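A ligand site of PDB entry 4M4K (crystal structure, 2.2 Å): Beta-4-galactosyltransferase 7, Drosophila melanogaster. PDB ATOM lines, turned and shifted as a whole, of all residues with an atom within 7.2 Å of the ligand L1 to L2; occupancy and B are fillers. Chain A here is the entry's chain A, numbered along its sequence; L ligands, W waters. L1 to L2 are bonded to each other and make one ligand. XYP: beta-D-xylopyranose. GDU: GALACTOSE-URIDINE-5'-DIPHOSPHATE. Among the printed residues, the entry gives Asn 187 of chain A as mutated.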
ATOM      1  N   ARG A  99      19.587  -3.538  -5.175  1.00  0.00           N
ATOM      2  CA  ARG A  99      19.940  -4.912  -4.860  1.00  0.00           C
ATOM      3  C   ARG A  99      20.088  -5.772  -6.113  1.00  0.00           C
ATOM      4  O   ARG A  99      21.059  -6.520  -6.284  1.00  0.00           O
ATOM      5  CB  ARG A  99      18.840  -5.491  -3.956  1.00  0.00           C
ATOM      6  CG  ARG A  99      19.043  -6.930  -3.570  1.00  0.00           C
ATOM      7  CD  ARG A  99      17.748  -7.582  -3.073  1.00  0.00           C
ATOM      8  NE  ARG A  99      18.044  -8.924  -2.599  1.00  0.00           N
ATOM      9  CZ  ARG A  99      17.386 -10.023  -2.940  1.00  0.00           C
ATOM     10  NH1 ARG A  99      16.356  -9.979  -3.781  1.00  0.00           N
ATOM     11  NH2 ARG A  99      17.777 -11.187  -2.426  1.00  0.00           N
ATOM     12  N   ASP A 121      20.311 -11.865   1.501  1.00  0.00           N
ATOM     13  CA  ASP A 121      20.307 -10.744   2.424  1.00  0.00           C
ATOM     14  C   ASP A 121      21.363 -10.915   3.512  1.00  0.00           C
ATOM     15  O   ASP A 121      21.589 -12.028   3.988  1.00  0.00           O
ATOM     16  CB  ASP A 121      18.942 -10.590   3.076  1.00  0.00           C
ATOM     17  CG  ASP A 121      17.846 -10.300   2.080  1.00  0.00           C
ATOM     18  OD1 ASP A 121      18.136 -10.109   0.867  1.00  0.00           O
ATOM     19  OD2 ASP A 121      16.681 -10.247   2.517  1.00  0.00           O
ATOM     20  N   HIS A 150       9.696 -17.732   6.616  1.00  0.00           N
ATOM     21  CA  HIS A 150      10.200 -16.372   6.833  1.00  0.00           C
ATOM     22  C   HIS A 150       9.408 -15.660   7.946  1.00  0.00           C
ATOM     23  O   HIS A 150       8.178 -15.747   7.991  1.00  0.00           O
ATOM     24  CB  HIS A 150      10.154 -15.572   5.530  1.00  0.00           C
ATOM     25  CG  HIS A 150      10.964 -14.321   5.556  1.00  0.00           C
ATOM     26  ND1 HIS A 150      10.536 -13.165   6.176  1.00  0.00           N
ATOM     27  CD2 HIS A 150      12.194 -14.042   5.063  1.00  0.00           C
ATOM     28  CE1 HIS A 150      11.453 -12.232   6.063  1.00  0.00           C
ATOM     29  NE2 HIS A 150      12.482 -12.740   5.388  1.00  0.00           N
ATOM     30  N   LYS A 152       8.639 -12.626   8.376  1.00  0.00           N
ATOM     31  CA  LYS A 152       7.937 -11.389   8.052  1.00  0.00           C
ATOM     32  C   LYS A 152       7.111 -11.467   6.774  1.00  0.00           C
ATOM     33  O   LYS A 152       6.029 -10.888   6.694  1.00  0.00           O
ATOM     34  CB  LYS A 152       8.951 -10.232   7.959  1.00  0.00           C
ATOM     35  CG  LYS A 152       8.352  -8.847   7.793  1.00  0.00           C
ATOM     36  CD  LYS A 152       9.436  -7.786   7.899  1.00  0.00           C
ATOM     37  CE  LYS A 152       8.935  -6.421   7.464  1.00  0.00           C
ATOM     38  NZ  LYS A 152       7.956  -5.866   8.423  1.00  0.00           N
ATOM     39  N   TYR A 153       7.619 -12.175   5.767  1.00  0.00           N
ATOM     40  CA  TYR A 153       6.955 -12.197   4.460  1.00  0.00           C
ATOM     41  C   TYR A 153       6.356 -13.541   4.156  1.00  0.00           C
ATOM     42  O   TYR A 153       7.074 -14.551   4.099  1.00  0.00           O
ATOM     43  CB  TYR A 153       7.951 -11.784   3.365  1.00  0.00           C
ATOM     44  CG  TYR A 153       8.545 -10.423   3.628  1.00  0.00           C
ATOM     45  CD1 TYR A 153       7.730  -9.302   3.747  1.00  0.00           C
ATOM     46  CD2 TYR A 153       9.919 -10.249   3.733  1.00  0.00           C
ATOM     47  CE1 TYR A 153       8.261  -8.040   3.975  1.00  0.00           C
ATOM     48  CE2 TYR A 153      10.465  -9.002   3.967  1.00  0.00           C
ATOM     49  CZ  TYR A 153       9.631  -7.903   4.079  1.00  0.00           C
ATOM     50  OH  TYR A 153      10.175  -6.670   4.318  1.00  0.00           O
ATOM     51  N   HIS A 154       5.045 -13.572   3.942  1.00  0.00           N
ATOM     52  CA  HIS A 154       4.296 -14.809   3.962  1.00  0.00           C
ATOM     53  C   HIS A 154       3.395 -14.987   2.735  1.00  0.00           C
ATOM     54  O   HIS A 154       2.615 -15.933   2.665  1.00  0.00           O
ATOM     55  CB  HIS A 154       3.458 -14.898   5.249  1.00  0.00           C
ATOM     56  CG  HIS A 154       4.251 -14.684   6.494  1.00  0.00           C
ATOM     57  ND1 HIS A 154       3.907 -13.734   7.445  1.00  0.00           N
ATOM     58  CD2 HIS A 154       5.365 -15.288   6.971  1.00  0.00           C
ATOM     59  CE1 HIS A 154       4.786 -13.767   8.432  1.00  0.00           C
ATOM     60  NE2 HIS A 154       5.682 -14.712   8.176  1.00  0.00           N
ATOM     61  N   TYR A 155       3.484 -14.081   1.774  1.00  0.00           N
ATOM     62  CA  TYR A 155       2.713 -14.293   0.546  1.00  0.00           C
ATOM     63  C   TYR A 155       3.333 -15.420  -0.285  1.00  0.00           C
ATOM     64  O   TYR A 155       4.547 -15.634  -0.248  1.00  0.00           O
ATOM     65  CB  TYR A 155       2.534 -12.996  -0.264  1.00  0.00           C
ATOM     66  CG  TYR A 155       3.809 -12.305  -0.741  1.00  0.00           C
ATOM     67  CD1 TYR A 155       4.555 -11.497   0.110  1.00  0.00           C
ATOM     68  CD2 TYR A 155       4.227 -12.429  -2.076  1.00  0.00           C
ATOM     69  CE1 TYR A 155       5.699 -10.849  -0.333  1.00  0.00           C
ATOM     70  CE2 TYR A 155       5.355 -11.776  -2.534  1.00  0.00           C
ATOM     71  CZ  TYR A 155       6.098 -10.985  -1.665  1.00  0.00           C
ATOM     72  OH  TYR A 155       7.240 -10.340  -2.094  1.00  0.00           O
ATOM     73  N   PHE A 158       6.465 -15.038  -2.645  1.00  0.00           N
ATOM     74  CA  PHE A 158       7.637 -14.380  -2.073  1.00  0.00           C
ATOM     75  C   PHE A 158       8.866 -15.233  -2.396  1.00  0.00           C
ATOM     76  O   PHE A 158       8.913 -16.410  -2.040  1.00  0.00           O
ATOM     77  CB  PHE A 158       7.496 -14.202  -0.558  1.00  0.00           C
ATOM     78  CG  PHE A 158       8.760 -13.758   0.119  1.00  0.00           C
ATOM     79  CD1 PHE A 158       9.225 -12.447  -0.021  1.00  0.00           C
ATOM     80  CD2 PHE A 158       9.490 -14.636   0.910  1.00  0.00           C
ATOM     81  CE1 PHE A 158      10.397 -12.027   0.604  1.00  0.00           C
ATOM     82  CE2 PHE A 158      10.654 -14.226   1.547  1.00  0.00           C
ATOM     83  CZ  PHE A 158      11.114 -12.920   1.392  1.00  0.00           C
ATOM     84  N   VAL A 159       9.838 -14.642  -3.094  1.00  0.00           N
ATOM     85  CA  VAL A 159      11.099 -15.336  -3.352  1.00  0.00           C
ATOM     86  C   VAL A 159      12.266 -14.483  -2.901  1.00  0.00           C
ATOM     87  O   VAL A 159      13.376 -14.614  -3.418  1.00  0.00           O
ATOM     88  CB  VAL A 159      11.273 -15.744  -4.845  1.00  0.00           C
ATOM     89  CG1 VAL A 159      10.244 -16.809  -5.235  1.00  0.00           C
ATOM     90  CG2 VAL A 159      11.170 -14.535  -5.773  1.00  0.00           C
ATOM     91  N   GLY A 160      12.032 -13.615  -1.918  1.00  0.00           N
ATOM     92  CA  GLY A 160      13.085 -12.755  -1.428  1.00  0.00           C
ATOM     93  C   GLY A 160      13.972 -13.410  -0.384  1.00  0.00           C
ATOM     94  O   GLY A 160      13.847 -14.615  -0.105  1.00  0.00           O
ATOM     95  N   GLY A 161      14.891 -12.631   0.183  1.00  0.00           N
ATOM     96  CA  GLY A 161      15.723 -13.097   1.273  1.00  0.00           C
ATOM     97  C   GLY A 161      16.855 -14.009   0.840  1.00  0.00           C
ATOM     98  O   GLY A 161      18.022 -13.602   0.845  1.00  0.00           O
ATOM     99  N   TRP A 183      14.073   0.242  -1.956  1.00  0.00           N
ATOM    100  CA  TRP A 183      13.466  -0.978  -1.466  1.00  0.00           C
ATOM    101  C   TRP A 183      12.303  -1.488  -2.319  1.00  0.00           C
ATOM    102  O   TRP A 183      11.463  -0.702  -2.800  1.00  0.00           O
ATOM    103  CB  TRP A 183      12.976  -0.760  -0.040  1.00  0.00           C
ATOM    104  CG  TRP A 183      12.347  -1.993   0.604  1.00  0.00           C
ATOM    105  CD1 TRP A 183      12.977  -2.911   1.413  1.00  0.00           C
ATOM    106  CD2 TRP A 183      10.980  -2.427   0.513  1.00  0.00           C
ATOM    107  NE1 TRP A 183      12.094  -3.881   1.820  1.00  0.00           N
ATOM    108  CE2 TRP A 183      10.861  -3.608   1.284  1.00  0.00           C
ATOM    109  CE3 TRP A 183       9.847  -1.926  -0.154  1.00  0.00           C
ATOM    110  CZ2 TRP A 183       9.648  -4.299   1.398  1.00  0.00           C
ATOM    111  CZ3 TRP A 183       8.638  -2.613  -0.025  1.00  0.00           C
ATOM    112  CH2 TRP A 183       8.549  -3.793   0.743  1.00  0.00           C
ATOM    113  N   GLY A 184      12.269  -2.811  -2.517  1.00  0.00           N
ATOM    114  CA  GLY A 184      11.056  -3.486  -2.908  1.00  0.00           C
ATOM    115  C   GLY A 184      10.869  -3.855  -4.362  1.00  0.00           C
ATOM    116  O   GLY A 184      11.445  -3.216  -5.263  1.00  0.00           O
ATOM    117  N   LEU A 185      10.057  -4.903  -4.550  1.00  0.00           N
ATOM    118  CA  LEU A 185       9.535  -5.363  -5.842  1.00  0.00           C
ATOM    119  C   LEU A 185      10.510  -6.129  -6.735  1.00  0.00           C
ATOM    120  O   LEU A 185      10.068  -6.894  -7.586  1.00  0.00           O
ATOM    121  CB  LEU A 185       8.872  -4.230  -6.625  1.00  0.00           C
ATOM    122  CG  LEU A 185       7.593  -3.657  -6.010  1.00  0.00           C
ATOM    123  CD1 LEU A 185       7.122  -2.473  -6.848  1.00  0.00           C
ATOM    124  CD2 LEU A 185       6.495  -4.739  -5.911  1.00  0.00           C
ATOM    125  N   GLU A 186      11.817  -5.963  -6.545  1.00  0.00           N
ATOM    126  CA  GLU A 186      12.786  -6.574  -7.472  1.00  0.00           C
ATOM    127  C   GLU A 186      12.649  -8.099  -7.513  1.00  0.00           C
ATOM    128  O   GLU A 186      12.685  -8.704  -8.589  1.00  0.00           O
ATOM    129  CB  GLU A 186      14.234  -6.106  -7.190  1.00  0.00           C
ATOM    130  CG  GLU A 186      15.016  -6.912  -6.153  1.00  0.00           C
ATOM    131  CD  GLU A 186      14.421  -6.843  -4.748  1.00  0.00           C
ATOM    132  OE1 GLU A 186      13.798  -5.799  -4.405  1.00  0.00           O
ATOM    133  OE2 GLU A 186      14.562  -7.827  -3.987  1.00  0.00           O
ATOM    134  N   ASN A 187      12.445  -8.712  -6.353  1.00  0.00           N
ATOM    135  CA  ASN A 187      12.243 -10.159  -6.277  1.00  0.00           C
ATOM    136  C   ASN A 187      10.910 -10.614  -6.855  1.00  0.00           C
ATOM    137  O   ASN A 187      10.803 -11.729  -7.375  1.00  0.00           O
ATOM    138  CB  ASN A 187      12.334 -10.632  -4.823  1.00  0.00           C
ATOM    139  CG  ASN A 187      11.466  -9.824  -3.888  1.00  0.00           C
ATOM    140  OD1 ASN A 187      11.371  -8.589  -4.019  1.00  0.00           O
ATOM    141  ND2 ASN A 187      10.829 -10.494  -2.927  1.00  0.00           N
ATOM    142  N   ASP A 188       9.889  -9.766  -6.771  1.00  0.00           N
ATOM    143  CA  ASP A 188       8.564 -10.110  -7.282  1.00  0.00           C
ATOM    144  C   ASP A 188       8.537 -10.145  -8.810  1.00  0.00           C
ATOM    145  O   ASP A 188       7.832 -10.968  -9.412  1.00  0.00           O
ATOM    146  CB  ASP A 188       7.540  -9.081  -6.785  1.00  0.00           C
ATOM    147  CG  ASP A 188       7.419  -9.084  -5.282  1.00  0.00           C
ATOM    148  OD1 ASP A 188       7.514 -10.162  -4.669  1.00  0.00           O
ATOM    149  OD2 ASP A 188       7.227  -7.989  -4.713  1.00  0.00           O
ATOM    150  N   ARG A 239       6.069  -1.329 -10.991  1.00  0.00           N
ATOM    151  CA  ARG A 239       5.021  -2.338 -10.828  1.00  0.00           C
ATOM    152  C   ARG A 239       4.735  -3.130 -12.102  1.00  0.00           C
ATOM    153  O   ARG A 239       3.847  -3.988 -12.138  1.00  0.00           O
ATOM    154  CB  ARG A 239       3.702  -1.729 -10.304  1.00  0.00           C
ATOM    155  CG  ARG A 239       3.811  -1.201  -8.864  1.00  0.00           C
ATOM    156  CD  ARG A 239       2.458  -1.187  -8.152  1.00  0.00           C
ATOM    157  NE  ARG A 239       2.640  -1.176  -6.691  1.00  0.00           N
ATOM    158  CZ  ARG A 239       2.881  -2.258  -5.953  1.00  0.00           C
ATOM    159  NH1 ARG A 239       2.972  -3.467  -6.528  1.00  0.00           N
ATOM    160  NH2 ARG A 239       3.034  -2.162  -4.639  1.00  0.00           N
HETATM  161  O1  XYP L   1       0.982  -7.013   0.832  1.00  0.00           O
HETATM  162  C1  XYP L   1       2.251  -6.489   0.510  1.00  0.00           C
HETATM  163  C2  XYP L   1       3.245  -6.961   1.544  1.00  0.00           C
HETATM  164  C3  XYP L   1       4.590  -6.446   1.207  1.00  0.00           C
HETATM  165  C4  XYP L   1       5.004  -6.917  -0.112  1.00  0.00           C
HETATM  166  C5  XYP L   1       4.021  -6.517  -1.174  1.00  0.00           C
HETATM  167  O2  XYP L   1       2.846  -6.472   2.853  1.00  0.00           O
HETATM  168  O3  XYP L   1       5.563  -6.913   2.152  1.00  0.00           O
HETATM  169  O4  XYP L   1       6.273  -6.260  -0.371  1.00  0.00           O
HETATM  170  O5  XYP L   1       2.632  -6.910  -0.831  1.00  0.00           O
HETATM  171  C1  XYP L   2       7.240  -7.207  -0.648  1.00  0.00           C
HETATM  172  C2  XYP L   2       8.297  -6.540  -1.532  1.00  0.00           C
HETATM  173  C3  XYP L   2       9.403  -7.484  -1.778  1.00  0.00           C
HETATM  174  C4  XYP L   2      10.018  -7.918  -0.511  1.00  0.00           C
HETATM  175  C5  XYP L   2       8.967  -8.542   0.441  1.00  0.00           C
HETATM  176  O2  XYP L   2       7.670  -6.121  -2.760  1.00  0.00           O
HETATM  177  O3  XYP L   2      10.392  -6.863  -2.628  1.00  0.00           O
HETATM  178  O4  XYP L   2      11.034  -8.911  -0.740  1.00  0.00           O
HETATM  179  O5  XYP L   2       7.793  -7.680   0.612  1.00  0.00           O
HETATM  180  N1  GDU L   3      20.894  -3.900   1.907  1.00  0.00           N
HETATM  181  C2  GDU L   3      21.999  -3.179   2.200  1.00  0.00           C
HETATM  182  N3  GDU L   3      21.964  -1.866   2.360  1.00  0.00           N
HETATM  183  C4  GDU L   3      20.808  -1.185   2.213  1.00  0.00           C
HETATM  184  C5  GDU L   3      19.625  -1.895   1.891  1.00  0.00           C
HETATM  185  C6  GDU L   3      19.717  -3.294   1.749  1.00  0.00           C
HETATM  186  O2  GDU L   3      23.058  -3.767   2.333  1.00  0.00           O
HETATM  187  O4  GDU L   3      20.748   0.206   2.371  1.00  0.00           O
HETATM  188  C1D GDU L   3      20.988  -5.271   1.713  1.00  0.00           C
HETATM  189  C2D GDU L   3      21.083  -6.141   2.964  1.00  0.00           C
HETATM  190  O2D GDU L   3      21.790  -7.288   2.573  1.00  0.00           O
HETATM  191  C3D GDU L   3      19.683  -6.435   3.238  1.00  0.00           C
HETATM  192  C4D GDU L   3      19.202  -6.759   1.876  1.00  0.00           C
HETATM  193  O4D GDU L   3      19.818  -5.778   1.005  1.00  0.00           O
HETATM  194  O3D GDU L   3      19.512  -7.516   4.154  1.00  0.00           O
HETATM  195  C5D GDU L   3      17.696  -6.644   1.764  1.00  0.00           C
HETATM  196  O5D GDU L   3      17.328  -5.350   2.164  1.00  0.00           O
HETATM  197  PA  GDU L   3      16.443  -5.133   3.494  1.00  0.00           P
HETATM  198  O1A GDU L   3      16.888  -6.090   4.622  1.00  0.00           O
HETATM  199  O2A GDU L   3      16.626  -3.702   3.934  1.00  0.00           O
HETATM  200  O3A GDU L   3      14.881  -5.394   3.146  1.00  0.00           O
HETATM  201  PB  GDU L   3      13.948  -6.539   3.730  1.00  0.00           P
HETATM  202  O1B GDU L   3      14.339  -6.899   5.191  1.00  0.00           O
HETATM  203  O2B GDU L   3      12.519  -6.034   3.698  1.00  0.00           O
HETATM  204  O3B GDU L   3      14.101  -7.854   2.814  1.00  0.00           O
HETATM  205  C1' GDU L   3      13.196  -8.177   1.760  1.00  0.00           C
HETATM  206  C2' GDU L   3      13.800  -9.241   0.997  1.00  0.00           C
HETATM  207  C3' GDU L   3      14.923  -8.744   0.246  1.00  0.00           C
HETATM  208  C4' GDU L   3      14.493  -7.788  -0.786  1.00  0.00           C
HETATM  209  C5' GDU L   3      13.889  -6.471  -0.124  1.00  0.00           C
HETATM  210  C6' GDU L   3      13.228  -5.677  -1.027  1.00  0.00           C
HETATM  211  O2' GDU L   3      14.290 -10.299   2.001  1.00  0.00           O
HETATM  212  O3' GDU L   3      15.691  -9.881  -0.360  1.00  0.00           O
HETATM  213  O4' GDU L   3      13.507  -8.442  -1.604  1.00  0.00           O
HETATM  214  O5' GDU L   3      12.912  -6.938   0.998  1.00  0.00           O
HETATM  215  O6' GDU L   3      14.073  -4.995  -1.736  1.00  0.00           O
HETATM  216  O   HOH W   1       3.296  -4.346  -3.533  1.00  0.00           O
HETATM  217  O   HOH W   2       5.917  -3.881  -2.377  1.00  0.00           O
HETATM  218  O   HOH W   3       4.851  -3.152  -0.189  1.00  0.00           O
HETATM  219  O   HOH W   4       2.858  -9.008  -2.754  1.00  0.00           O
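O4 of XYP L2 sits at hydrogen-bond distance from O4' of GDU L3.
CE1 of Tyr 153 touches O5 of XYP L2 (3.4 Å). OH of Tyr 155 touches C1 of XYP L2 (3.5 Å). Phe 158 touches the ligand L1 to L2. CH2 of Trp 183 touches O4 of XYP L1, at 3.5 Å. CA of Gly 184 touches O3 of XYP L2, at 3.5 Å. OE1 of Glu 186 touches O3 of XYP L2, at 3.99 Å. Hydrophobic or aromatic side chains that line the ligand L1 to L2: Tyr 153, Tyr 155, Phe 158, Trp 183 and Leu 185. The nearest printed residue that does not touch the ligand L1 to L2 is Gly 160 (4.4 Å).
OD2 of Asp 188 lies within hydrogen-bond range of O2 of XYP L2, at 2.7 Å. The backbone NH (N) of Gly 184 is in hydrogen-bond range of an oxygen (O6') of GDU L3, at 2.9 Å. OE2 of Glu 186 is in hydrogen-bond range of O4' of GDU L3, at 2.7 Å. An oxygen (O3') of GDU L3 lies close to the guanidinium group (NH2) of Arg 99. NE1 of Trp 183 lies within hydrogen-bond range of O2B of GDU L3, at 2.9 Å. O3' of GDU L3 is in hydrogen-bond range of N of Gly 161. OD1 of Asn 187 is in hydrogen-bond range of O3 of XYP L2 (2.4 Å). The side-chain amide oxygen of Asn 187 is in hydrogen-bond range of an oxygen (O4') of GDU L3 (3.2 Å). O3 of XYP L2 sits at hydrogen-bond distance from N of Leu 185. The side-chain carboxylate (OD2) of Asp 121 lies within hydrogen-bond range of an oxygen (O2') of GDU L3. The side-chain hydroxyl of Tyr 153 sits at hydrogen-bond distance from an oxygen (O2B) of GDU L3.
The side-chain hydroxyl (OH) of Tyr 155 sits at hydrogen-bond distance from the side-chain carboxylate (OD1) of Asp 188 (2.6 Å). OD1 of Asn 187 sits close to OE2 of Glu 186. A ring nitrogen (ND1) of His 150 is in hydrogen-bond range of the backbone NH (N) of Tyr 153 (3.1 Å). N of Gly 160 lies close to ND2 of Asn 187, 3.5 Å away. NH1 of Arg 99 lies within salt-bridge range of OE2 of Glu 186 (2.8 Å).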
